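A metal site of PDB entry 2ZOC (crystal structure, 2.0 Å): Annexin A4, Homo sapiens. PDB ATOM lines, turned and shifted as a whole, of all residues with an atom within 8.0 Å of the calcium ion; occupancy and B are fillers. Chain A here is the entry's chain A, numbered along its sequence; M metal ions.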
ATOM      1  N   TYR A 255     -12.505  -9.034  10.245  1.00  0.00           N
ATOM      2  CA  TYR A 255     -11.595  -9.827  11.061  1.00  0.00           C
ATOM      3  C   TYR A 255     -11.918 -11.308  10.888  1.00  0.00           C
ATOM      4  O   TYR A 255     -11.055 -12.099  10.540  1.00  0.00           O
ATOM      5  CB  TYR A 255     -11.741  -9.440  12.529  1.00  0.00           C
ATOM      6  CG  TYR A 255     -10.953 -10.314  13.486  1.00  0.00           C
ATOM      7  CD1 TYR A 255      -9.584 -10.135  13.660  1.00  0.00           C
ATOM      8  CD2 TYR A 255     -11.586 -11.320  14.212  1.00  0.00           C
ATOM      9  CE1 TYR A 255      -8.862 -10.939  14.546  1.00  0.00           C
ATOM     10  CE2 TYR A 255     -10.880 -12.137  15.085  1.00  0.00           C
ATOM     11  CZ  TYR A 255      -9.518 -11.935  15.252  1.00  0.00           C
ATOM     12  OH  TYR A 255      -8.819 -12.734  16.132  1.00  0.00           O
ATOM     13  N   LYS A 256     -13.176 -11.661  11.126  1.00  0.00           N
ATOM     14  CA  LYS A 256     -13.611 -13.044  11.027  1.00  0.00           C
ATOM     15  C   LYS A 256     -13.458 -13.641   9.636  1.00  0.00           C
ATOM     16  O   LYS A 256     -13.318 -14.865   9.510  1.00  0.00           O
ATOM     17  CB  LYS A 256     -15.081 -13.169  11.460  1.00  0.00           C
ATOM     18  CG  LYS A 256     -15.347 -12.773  12.899  1.00  0.00           C
ATOM     19  CD  LYS A 256     -16.808 -12.995  13.240  1.00  0.00           C
ATOM     20  CE  LYS A 256     -17.087 -12.653  14.688  1.00  0.00           C
ATOM     21  NZ  LYS A 256     -16.364 -13.579  15.593  1.00  0.00           N
ATOM     22  N   SER A 257     -13.475 -12.809   8.604  1.00  0.00           N
ATOM     23  CA  SER A 257     -13.346 -13.300   7.240  1.00  0.00           C
ATOM     24  C   SER A 257     -11.916 -13.686   6.870  1.00  0.00           C
ATOM     25  O   SER A 257     -11.689 -14.423   5.912  1.00  0.00           O
ATOM     26  CB  SER A 257     -13.872 -12.251   6.249  1.00  0.00           C
ATOM     27  OG  SER A 257     -13.042 -11.091   6.234  1.00  0.00           O
ATOM     28  N   MET A 258     -10.954 -13.190   7.636  1.00  0.00           N
ATOM     29  CA  MET A 258      -9.569 -13.483   7.364  1.00  0.00           C
ATOM     30  C   MET A 258      -8.877 -14.307   8.446  1.00  0.00           C
ATOM     31  O   MET A 258      -7.941 -15.047   8.158  1.00  0.00           O
ATOM     32  CB  MET A 258      -8.791 -12.173   7.149  1.00  0.00           C
ATOM     33  CG  MET A 258      -9.294 -11.368   5.955  1.00  0.00           C
ATOM     34  SD  MET A 258      -8.429  -9.794   5.770  1.00  0.00           S
ATOM     35  CE  MET A 258      -9.519  -8.702   6.698  1.00  0.00           C
ATOM     36  N   LYS A 259      -9.340 -14.175   9.687  1.00  0.00           N
ATOM     37  CA  LYS A 259      -8.715 -14.915  10.779  1.00  0.00           C
ATOM     38  C   LYS A 259      -8.845 -16.429  10.594  1.00  0.00           C
ATOM     39  O   LYS A 259      -9.944 -16.954  10.409  1.00  0.00           O
ATOM     40  CB  LYS A 259      -9.320 -14.504  12.128  1.00  0.00           C
ATOM     41  CG  LYS A 259      -8.499 -14.979  13.328  1.00  0.00           C
ATOM     42  CD  LYS A 259      -7.073 -14.424  13.271  1.00  0.00           C
ATOM     43  CE  LYS A 259      -6.271 -14.794  14.505  1.00  0.00           C
ATOM     44  NZ  LYS A 259      -6.110 -16.265  14.654  1.00  0.00           N
ATOM     45  N   GLY A 260      -7.712 -17.119  10.641  1.00  0.00           N
ATOM     46  CA  GLY A 260      -7.739 -18.561  10.464  1.00  0.00           C
ATOM     47  C   GLY A 260      -7.261 -18.940   9.080  1.00  0.00           C
ATOM     48  O   GLY A 260      -6.945 -18.071   8.265  1.00  0.00           O
ATOM     49  N   LEU A 261      -7.218 -20.242   8.822  1.00  0.00           N
ATOM     50  CA  LEU A 261      -6.764 -20.747   7.533  1.00  0.00           C
ATOM     51  C   LEU A 261      -7.645 -20.271   6.385  1.00  0.00           C
ATOM     52  O   LEU A 261      -8.854 -20.450   6.404  1.00  0.00           O
ATOM     53  CB  LEU A 261      -6.734 -22.267   7.554  1.00  0.00           C
ATOM     54  CG  LEU A 261      -6.348 -22.997   6.273  1.00  0.00           C
ATOM     55  CD1 LEU A 261      -4.953 -22.600   5.826  1.00  0.00           C
ATOM     56  CD2 LEU A 261      -6.401 -24.504   6.526  1.00  0.00           C
ATOM     57  N   GLY A 262      -7.016 -19.679   5.366  1.00  0.00           N
ATOM     58  CA  GLY A 262      -7.770 -19.219   4.214  1.00  0.00           C
ATOM     59  C   GLY A 262      -8.539 -17.925   4.398  1.00  0.00           C
ATOM     60  O   GLY A 262      -8.299 -17.183   5.350  1.00  0.00           O
ATOM     61  N   THR A 263      -9.466 -17.664   3.492  1.00  0.00           N
ATOM     62  CA  THR A 263     -10.245 -16.439   3.549  1.00  0.00           C
ATOM     63  C   THR A 263     -11.675 -16.610   3.058  1.00  0.00           C
ATOM     64  O   THR A 263     -11.925 -17.343   2.102  1.00  0.00           O
ATOM     65  CB  THR A 263      -9.609 -15.344   2.653  1.00  0.00           C
ATOM     66  OG1 THR A 263      -8.200 -15.283   2.879  1.00  0.00           O
ATOM     67  CG2 THR A 263     -10.247 -13.991   2.938  1.00  0.00           C
ATOM     68  N   ASP A 264     -12.613 -15.946   3.742  1.00  0.00           N
ATOM     69  CA  ASP A 264     -14.006 -15.951   3.333  1.00  0.00           C
ATOM     70  C   ASP A 264     -13.967 -14.776   2.362  1.00  0.00           C
ATOM     71  O   ASP A 264     -14.214 -13.640   2.748  1.00  0.00           O
ATOM     72  CB  ASP A 264     -14.937 -15.637   4.510  1.00  0.00           C
ATOM     73  CG  ASP A 264     -16.391 -15.475   4.082  1.00  0.00           C
ATOM     74  OD1 ASP A 264     -16.680 -15.518   2.874  1.00  0.00           O
ATOM     75  OD2 ASP A 264     -17.258 -15.282   4.961  1.00  0.00           O
ATOM     76  N   PHE A 298      -3.957  -7.279   7.986  1.00  0.00           N
ATOM     77  CA  PHE A 298      -4.728  -8.496   7.736  1.00  0.00           C
ATOM     78  C   PHE A 298      -4.949  -8.746   6.249  1.00  0.00           C
ATOM     79  O   PHE A 298      -4.747  -9.864   5.770  1.00  0.00           O
ATOM     80  CB  PHE A 298      -6.087  -8.441   8.439  1.00  0.00           C
ATOM     81  CG  PHE A 298      -6.083  -9.038   9.822  1.00  0.00           C
ATOM     82  CD1 PHE A 298      -5.383  -8.444  10.859  1.00  0.00           C
ATOM     83  CD2 PHE A 298      -6.783 -10.220  10.082  1.00  0.00           C
ATOM     84  CE1 PHE A 298      -5.377  -8.999  12.138  1.00  0.00           C
ATOM     85  CE2 PHE A 298      -6.780 -10.789  11.362  1.00  0.00           C
ATOM     86  CZ  PHE A 298      -6.077 -10.176  12.384  1.00  0.00           C
ATOM     87  N   GLY A 301      -1.740  -9.845   4.624  1.00  0.00           N
ATOM     88  CA  GLY A 301      -1.358 -11.190   5.024  1.00  0.00           C
ATOM     89  C   GLY A 301      -2.283 -12.302   4.555  1.00  0.00           C
ATOM     90  O   GLY A 301      -1.895 -13.467   4.562  1.00  0.00           O
ATOM     91  N   ASP A 302      -3.489 -11.958   4.119  1.00  0.00           N
ATOM     92  CA  ASP A 302      -4.452 -12.974   3.688  1.00  0.00           C
ATOM     93  C   ASP A 302      -4.698 -13.081   2.189  1.00  0.00           C
ATOM     94  O   ASP A 302      -5.315 -14.043   1.738  1.00  0.00           O
ATOM     95  CB  ASP A 302      -5.790 -12.736   4.380  1.00  0.00           C
ATOM     96  CG  ASP A 302      -6.134 -13.820   5.368  1.00  0.00           C
ATOM     97  OD1 ASP A 302      -5.345 -14.026   6.316  1.00  0.00           O
ATOM     98  OD2 ASP A 302      -7.181 -14.475   5.185  1.00  0.00           O
ATOM     99  N   THR A 303      -4.244 -12.089   1.432  1.00  0.00           N
ATOM    100  CA  THR A 303      -4.482 -12.092  -0.003  1.00  0.00           C
ATOM    101  C   THR A 303      -3.194 -11.811  -0.786  1.00  0.00           C
ATOM    102  O   THR A 303      -2.167 -11.470  -0.203  1.00  0.00           O
ATOM    103  CB  THR A 303      -5.539 -11.038  -0.375  1.00  0.00           C
ATOM    104  OG1 THR A 303      -4.959  -9.726  -0.272  1.00  0.00           O
ATOM    105  CG2 THR A 303      -6.729 -11.109   0.585  1.00  0.00           C
HETATM  106 CA    CA M   1      -6.699 -16.146   6.727  1.00  0.00          CA
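O of Asp 302 sits at hydrogen-bond distance from OG1 of Thr 263 (3.3 Å).
O of Met 258 is bound to the calcium ion (2.2 Å). OD2 of Asp 302 binds the calcium ion, at 2.3 Å. The calcium ion is bound by O of Gly 262 (2.4 Å). The backbone carbonyl oxygen (O) of Gly 260 is bound to the calcium ion (2.5 Å). The side-chain carboxylate (OD1) of Asp 302 is bound to the calcium ion (2.5 Å). The calcium ion has five donor atoms within binding distance.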
